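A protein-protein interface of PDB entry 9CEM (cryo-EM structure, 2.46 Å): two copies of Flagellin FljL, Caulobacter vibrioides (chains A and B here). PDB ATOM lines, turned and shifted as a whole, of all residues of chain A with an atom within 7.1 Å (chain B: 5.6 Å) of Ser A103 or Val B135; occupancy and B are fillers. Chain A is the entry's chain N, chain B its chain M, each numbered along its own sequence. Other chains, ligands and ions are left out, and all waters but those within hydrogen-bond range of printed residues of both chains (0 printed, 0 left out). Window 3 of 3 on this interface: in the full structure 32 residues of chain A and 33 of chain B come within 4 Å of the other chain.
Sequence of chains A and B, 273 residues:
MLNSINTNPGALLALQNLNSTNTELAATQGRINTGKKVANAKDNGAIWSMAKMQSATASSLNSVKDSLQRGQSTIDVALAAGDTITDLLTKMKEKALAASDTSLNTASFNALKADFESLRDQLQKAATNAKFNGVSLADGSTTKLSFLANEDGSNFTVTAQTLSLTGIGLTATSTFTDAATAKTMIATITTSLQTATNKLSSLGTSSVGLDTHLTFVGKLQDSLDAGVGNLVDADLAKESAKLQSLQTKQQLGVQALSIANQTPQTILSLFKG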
ATOM      1  N   SER A 100     -23.522   9.459 -25.097  1.00  0.00           N
ATOM      2  CA  SER A 100     -23.309   8.631 -26.282  1.00  0.00           C
ATOM      3  C   SER A 100     -21.915   8.797 -26.880  1.00  0.00           C
ATOM      4  O   SER A 100     -21.494   7.948 -27.674  1.00  0.00           O
ATOM      5  CB  SER A 100     -24.365   8.945 -27.338  1.00  0.00           C
ATOM      6  OG  SER A 100     -25.663   8.839 -26.788  1.00  0.00           O
ATOM      7  N   ASP A 101     -21.197   9.866 -26.536  1.00  0.00           N
ATOM      8  CA  ASP A 101     -19.894  10.126 -27.139  1.00  0.00           C
ATOM      9  C   ASP A 101     -18.896   9.035 -26.754  1.00  0.00           C
ATOM     10  O   ASP A 101     -18.834   8.611 -25.596  1.00  0.00           O
ATOM     11  CB  ASP A 101     -19.385  11.500 -26.700  1.00  0.00           C
ATOM     12  CG  ASP A 101     -18.087  11.899 -27.385  1.00  0.00           C
ATOM     13  OD1 ASP A 101     -17.707  13.084 -27.275  1.00  0.00           O
ATOM     14  OD2 ASP A 101     -17.448  11.055 -28.046  1.00  0.00           O
ATOM     15  N   THR A 102     -18.107   8.590 -27.737  1.00  0.00           N
ATOM     16  CA  THR A 102     -17.130   7.525 -27.537  1.00  0.00           C
ATOM     17  C   THR A 102     -15.859   8.003 -26.839  1.00  0.00           C
ATOM     18  O   THR A 102     -15.224   7.218 -26.125  1.00  0.00           O
ATOM     19  CB  THR A 102     -16.790   6.891 -28.895  1.00  0.00           C
ATOM     20  OG1 THR A 102     -17.922   6.154 -29.374  1.00  0.00           O
ATOM     21  CG2 THR A 102     -15.598   5.946 -28.800  1.00  0.00           C
ATOM     22  N   SER A 103     -15.501   9.277 -26.986  1.00  0.00           N
ATOM     23  CA  SER A 103     -14.237   9.793 -26.473  1.00  0.00           C
ATOM     24  C   SER A 103     -14.208   9.918 -24.956  1.00  0.00           C
ATOM     25  O   SER A 103     -13.128  10.123 -24.392  1.00  0.00           O
ATOM     26  CB  SER A 103     -13.930  11.156 -27.101  1.00  0.00           C
ATOM     27  OG  SER A 103     -15.070  11.997 -27.084  1.00  0.00           O
ATOM     28  N   LEU A 104     -15.355   9.818 -24.291  1.00  0.00           N
ATOM     29  CA  LEU A 104     -15.403   9.951 -22.841  1.00  0.00           C
ATOM     30  C   LEU A 104     -14.607   8.848 -22.154  1.00  0.00           C
ATOM     31  O   LEU A 104     -14.594   7.697 -22.598  1.00  0.00           O
ATOM     32  CB  LEU A 104     -16.850   9.910 -22.354  1.00  0.00           C
ATOM     33  CG  LEU A 104     -17.777  11.051 -22.761  1.00  0.00           C
ATOM     34  CD1 LEU A 104     -19.188  10.762 -22.283  1.00  0.00           C
ATOM     35  CD2 LEU A 104     -17.270  12.350 -22.168  1.00  0.00           C
ATOM     36  N   ASN A 105     -13.942   9.213 -21.060  1.00  0.00           N
ATOM     37  CA  ASN A 105     -13.356   8.237 -20.156  1.00  0.00           C
ATOM     38  C   ASN A 105     -14.437   7.689 -19.225  1.00  0.00           C
ATOM     39  O   ASN A 105     -15.558   8.202 -19.166  1.00  0.00           O
ATOM     40  CB  ASN A 105     -12.179   8.850 -19.394  1.00  0.00           C
ATOM     41  CG  ASN A 105     -12.581  10.022 -18.505  1.00  0.00           C
ATOM     42  OD1 ASN A 105     -13.761  10.257 -18.241  1.00  0.00           O
ATOM     43  ND2 ASN A 105     -11.585  10.763 -18.035  1.00  0.00           N
ATOM     44  N   THR A 106     -14.102   6.624 -18.494  1.00  0.00           N
ATOM     45  CA  THR A 106     -15.114   5.885 -17.743  1.00  0.00           C
ATOM     46  C   THR A 106     -15.774   6.749 -16.671  1.00  0.00           C
ATOM     47  O   THR A 106     -16.985   6.645 -16.434  1.00  0.00           O
ATOM     48  CB  THR A 106     -14.478   4.646 -17.108  1.00  0.00           C
ATOM     49  OG1 THR A 106     -13.619   4.006 -18.060  1.00  0.00           O
ATOM     50  CG2 THR A 106     -15.550   3.668 -16.658  1.00  0.00           C
ATOM     51  N   SER A 108     -16.349  10.009 -16.609  1.00  0.00           N
ATOM     52  CA  SER A 108     -17.304  10.966 -17.155  1.00  0.00           C
ATOM     53  C   SER A 108     -18.617  10.283 -17.504  1.00  0.00           C
ATOM     54  O   SER A 108     -19.700  10.809 -17.212  1.00  0.00           O
ATOM     55  CB  SER A 108     -16.711  11.641 -18.390  1.00  0.00           C
ATOM     56  OG  SER A 108     -15.410  12.134 -18.128  1.00  0.00           O
ATOM     57  N   SER B  67     -18.512  18.185 -27.410  1.00  0.00           N
ATOM     58  CA  SER B  67     -17.850  17.019 -27.987  1.00  0.00           C
ATOM     59  C   SER B  67     -16.853  17.428 -29.065  1.00  0.00           C
ATOM     60  O   SER B  67     -15.725  16.917 -29.108  1.00  0.00           O
ATOM     61  CB  SER B  67     -18.891  16.052 -28.549  1.00  0.00           C
ATOM     62  OG  SER B  67     -18.300  14.810 -28.885  1.00  0.00           O
ATOM     63  N   ARG B  70     -13.752  18.875 -27.283  1.00  0.00           N
ATOM     64  CA  ARG B  70     -12.855  17.869 -26.722  1.00  0.00           C
ATOM     65  C   ARG B  70     -12.121  17.094 -27.813  1.00  0.00           C
ATOM     66  O   ARG B  70     -10.940  16.753 -27.646  1.00  0.00           O
ATOM     67  CB  ARG B  70     -13.628  16.928 -25.796  1.00  0.00           C
ATOM     68  CG  ARG B  70     -12.738  15.930 -25.074  1.00  0.00           C
ATOM     69  CD  ARG B  70     -13.519  15.059 -24.101  1.00  0.00           C
ATOM     70  NE  ARG B  70     -14.491  14.203 -24.764  1.00  0.00           N
ATOM     71  CZ  ARG B  70     -15.804  14.326 -24.623  1.00  0.00           C
ATOM     72  NH1 ARG B  70     -16.331  15.247 -23.833  1.00  0.00           N
ATOM     73  NH2 ARG B  70     -16.608  13.501 -25.285  1.00  0.00           N
ATOM     74  N   THR B  74      -8.064  16.850 -28.418  1.00  0.00           N
ATOM     75  CA  THR B  74      -7.339  15.596 -28.600  1.00  0.00           C
ATOM     76  C   THR B  74      -6.465  15.640 -29.850  1.00  0.00           C
ATOM     77  O   THR B  74      -5.320  15.161 -29.836  1.00  0.00           O
ATOM     78  CB  THR B  74      -8.327  14.432 -28.665  1.00  0.00           C
ATOM     79  OG1 THR B  74      -9.077  14.373 -27.445  1.00  0.00           O
ATOM     80  CG2 THR B  74      -7.596  13.116 -28.858  1.00  0.00           C
ATOM     81  N   ALA B 130       1.237  10.374 -25.627  1.00  0.00           N
ATOM     82  CA  ALA B 130       0.263  11.274 -26.247  1.00  0.00           C
ATOM     83  C   ALA B 130      -1.152  10.827 -25.901  1.00  0.00           C
ATOM     84  O   ALA B 130      -1.714   9.936 -26.535  1.00  0.00           O
ATOM     85  CB  ALA B 130       0.460  11.312 -27.755  1.00  0.00           C
ATOM     86  N   LYS B 131      -1.744  11.466 -24.890  1.00  0.00           N
ATOM     87  CA  LYS B 131      -3.130  11.221 -24.508  1.00  0.00           C
ATOM     88  C   LYS B 131      -3.748  12.493 -23.948  1.00  0.00           C
ATOM     89  O   LYS B 131      -3.057  13.342 -23.381  1.00  0.00           O
ATOM     90  CB  LYS B 131      -3.267  10.098 -23.463  1.00  0.00           C
ATOM     91  CG  LYS B 131      -2.836   8.720 -23.928  1.00  0.00           C
ATOM     92  CD  LYS B 131      -3.073   7.677 -22.856  1.00  0.00           C
ATOM     93  CE  LYS B 131      -2.106   7.861 -21.704  1.00  0.00           C
ATOM     94  NZ  LYS B 131      -0.705   7.594 -22.131  1.00  0.00           N
ATOM     95  N   PHE B 132      -5.067  12.603 -24.102  1.00  0.00           N
ATOM     96  CA  PHE B 132      -5.851  13.711 -23.565  1.00  0.00           C
ATOM     97  C   PHE B 132      -7.015  13.138 -22.767  1.00  0.00           C
ATOM     98  O   PHE B 132      -7.962  12.600 -23.349  1.00  0.00           O
ATOM     99  CB  PHE B 132      -6.365  14.622 -24.678  1.00  0.00           C
ATOM    100  CG  PHE B 132      -7.133  15.809 -24.174  1.00  0.00           C
ATOM    101  CD1 PHE B 132      -6.480  16.870 -23.572  1.00  0.00           C
ATOM    102  CD2 PHE B 132      -8.512  15.848 -24.275  1.00  0.00           C
ATOM    103  CE1 PHE B 132      -7.188  17.956 -23.101  1.00  0.00           C
ATOM    104  CE2 PHE B 132      -9.224  16.930 -23.804  1.00  0.00           C
ATOM    105  CZ  PHE B 132      -8.561  17.986 -23.215  1.00  0.00           C
ATOM    106  N   ASN B 133      -6.948  13.271 -21.442  1.00  0.00           N
ATOM    107  CA  ASN B 133      -7.994  12.785 -20.540  1.00  0.00           C
ATOM    108  C   ASN B 133      -8.236  11.286 -20.754  1.00  0.00           C
ATOM    109  O   ASN B 133      -9.370  10.813 -20.839  1.00  0.00           O
ATOM    110  CB  ASN B 133      -9.278  13.614 -20.705  1.00  0.00           C
ATOM    111  CG  ASN B 133     -10.445  13.089 -19.883  1.00  0.00           C
ATOM    112  OD1 ASN B 133     -10.332  12.905 -18.671  1.00  0.00           O
ATOM    113  ND2 ASN B 133     -11.573  12.844 -20.543  1.00  0.00           N
ATOM    114  N   GLY B 134      -7.144  10.530 -20.870  1.00  0.00           N
ATOM    115  CA  GLY B 134      -7.207   9.084 -20.926  1.00  0.00           C
ATOM    116  C   GLY B 134      -7.549   8.480 -22.271  1.00  0.00           C
ATOM    117  O   GLY B 134      -7.748   7.261 -22.346  1.00  0.00           O
ATOM    118  N   VAL B 135      -7.626   9.280 -23.332  1.00  0.00           N
ATOM    119  CA  VAL B 135      -7.993   8.801 -24.658  1.00  0.00           C
ATOM    120  C   VAL B 135      -7.034   9.423 -25.665  1.00  0.00           C
ATOM    121  O   VAL B 135      -6.574  10.556 -25.487  1.00  0.00           O
ATOM    122  CB  VAL B 135      -9.467   9.138 -24.991  1.00  0.00           C
ATOM    123  CG1 VAL B 135      -9.815   8.732 -26.402  1.00  0.00           C
ATOM    124  CG2 VAL B 135     -10.407   8.458 -24.007  1.00  0.00           C
ATOM    125  N   SER B 136      -6.726   8.680 -26.728  1.00  0.00           N
ATOM    126  CA  SER B 136      -5.671   9.090 -27.642  1.00  0.00           C
ATOM    127  C   SER B 136      -5.995   8.666 -29.067  1.00  0.00           C
ATOM    128  O   SER B 136      -6.744   7.715 -29.302  1.00  0.00           O
ATOM    129  CB  SER B 136      -4.323   8.498 -27.225  1.00  0.00           C
ATOM    130  OG  SER B 136      -3.336   8.741 -28.211  1.00  0.00           O
ATOM    131  N   LEU B 137      -5.415   9.397 -30.021  1.00  0.00           N
ATOM    132  CA  LEU B 137      -5.501   9.064 -31.440  1.00  0.00           C
ATOM    133  C   LEU B 137      -4.148   8.788 -32.083  1.00  0.00           C
ATOM    134  O   LEU B 137      -4.071   8.699 -33.313  1.00  0.00           O
ATOM    135  CB  LEU B 137      -6.219  10.175 -32.210  1.00  0.00           C
ATOM    136  CG  LEU B 137      -7.691  10.359 -31.863  1.00  0.00           C
ATOM    137  CD1 LEU B 137      -8.259  11.558 -32.569  1.00  0.00           C
ATOM    138  CD2 LEU B 137      -8.424   9.111 -32.295  1.00  0.00           C
ATOM    139  N   LEU B 145     -12.264   7.346 -33.077  1.00  0.00           N
ATOM    140  CA  LEU B 145     -13.148   7.981 -32.110  1.00  0.00           C
ATOM    141  C   LEU B 145     -14.310   8.641 -32.833  1.00  0.00           C
ATOM    142  O   LEU B 145     -14.120   9.329 -33.841  1.00  0.00           O
ATOM    143  CB  LEU B 145     -12.421   9.028 -31.266  1.00  0.00           C
ATOM    144  CG  LEU B 145     -11.267   8.597 -30.373  1.00  0.00           C
ATOM    145  CD1 LEU B 145     -10.795   9.798 -29.585  1.00  0.00           C
ATOM    146  CD2 LEU B 145     -11.705   7.485 -29.441  1.00  0.00           C
ATOM    147  N   SER B 146     -15.510   8.428 -32.310  1.00  0.00           N
ATOM    148  CA  SER B 146     -16.709   9.099 -32.782  1.00  0.00           C
ATOM    149  C   SER B 146     -16.971  10.325 -31.921  1.00  0.00           C
ATOM    150  O   SER B 146     -16.767  10.294 -30.704  1.00  0.00           O
ATOM    151  CB  SER B 146     -17.912   8.155 -32.745  1.00  0.00           C
ATOM    152  OG  SER B 146     -17.712   7.048 -33.606  1.00  0.00           O
ATOM    153  N   PHE B 147     -17.420  11.402 -32.556  1.00  0.00           N
ATOM    154  CA  PHE B 147     -17.758  12.636 -31.866  1.00  0.00           C
ATOM    155  C   PHE B 147     -19.147  13.083 -32.296  1.00  0.00           C
ATOM    156  O   PHE B 147     -19.570  12.835 -33.427  1.00  0.00           O
ATOM    157  CB  PHE B 147     -16.741  13.752 -32.154  1.00  0.00           C
ATOM    158  CG  PHE B 147     -15.330  13.407 -31.765  1.00  0.00           C
ATOM    159  CD1 PHE B 147     -14.960  13.362 -30.433  1.00  0.00           C
ATOM    160  CD2 PHE B 147     -14.373  13.139 -32.729  1.00  0.00           C
ATOM    161  CE1 PHE B 147     -13.666  13.052 -30.070  1.00  0.00           C
ATOM    162  CE2 PHE B 147     -13.076  12.827 -32.369  1.00  0.00           C
ATOM    163  CZ  PHE B 147     -12.724  12.784 -31.038  1.00  0.00           C
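The guanidinium group (NH2) of Arg B70 lies within salt-bridge range of the side-chain carboxylate (OD2) of Asp A101 (3.8 Å).
The side-chain carboxylate of Asp A101 lies close to the backbone carbonyl oxygen of Ser B146, at 2.8 Å.
The side-chain hydroxyl (OG) of Ser B67 lies within hydrogen-bond range of the side-chain carboxylate (OD1) of Asp A101, 2.4 Å away.
The guanidinium group (NH2) of Arg B70 sits at hydrogen-bond distance from the side-chain hydroxyl (OG) of Ser A103 (2.8 Å).
The side-chain amide oxygen of Asn B133 lies within hydrogen-bond range of the side-chain amide nitrogen of Asn A105.
The side-chain hydroxyl (OG1) of Thr B74 sits at hydrogen-bond distance from the backbone carbonyl oxygen (O) of Arg B70.
The side-chain hydroxyl (OG) of Ser A103 sits at hydrogen-bond distance from the side-chain carboxylate (OD2) of Asp A101, 2.7 Å away.
The side-chain hydroxyl (OG) of Ser A108 is in hydrogen-bond range of the side-chain amide oxygen (OD1) of Asn A105 (2.5 Å).
Thr A102 touches Ser B146 (N to O, 3.7 Å).
O of Ser A103 touches CG2 of Val B135 (3.2 Å).
Ser A103 touches Phe B147 (OG to CE1, 3.5 Å).
Arg B70 touches Leu A104.
Of the printed residues of chain A, Val B135 touches Ser A103 (3.2 Å).
No residue of chain A comes within 4 Å of Gly B134.
Printed residues of chain B within 4 Å of Asn A105: Asn B133 (2.6 Å).
Printed residues of chain B within 4 Å of Leu A104: Arg B70.
Ser A100 touches none of the printed residues of chain B.
The nearest residue of chain A that does not touch Val B135 is Leu A104 (4.5 Å).
The nearest printed residue of chain A that does not touch Ser B67 is Ser A103 (4.6 Å).
Of the 14 printed residues of chain B, 6 touch a printed residue of chain A.
Of the 8 printed residues of chain A, 5 touch a printed residue of chain B.
Hydrophobic or aromatic side chains of chain A within 4 Å of the printed part of chain B: Leu A104.
Among the printed residues, 9 pairs touch across the chains.
Among the printed residues, Asp or Glu carboxylates within 4 Å of a Lys or Arg side-chain nitrogen of the other chain: Asp A101 with Arg B70.
No position is printed for both chains.
Of the 9 pairs that touch across the chains among the printed residues, none has its exchanged pair printed and touching as well.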
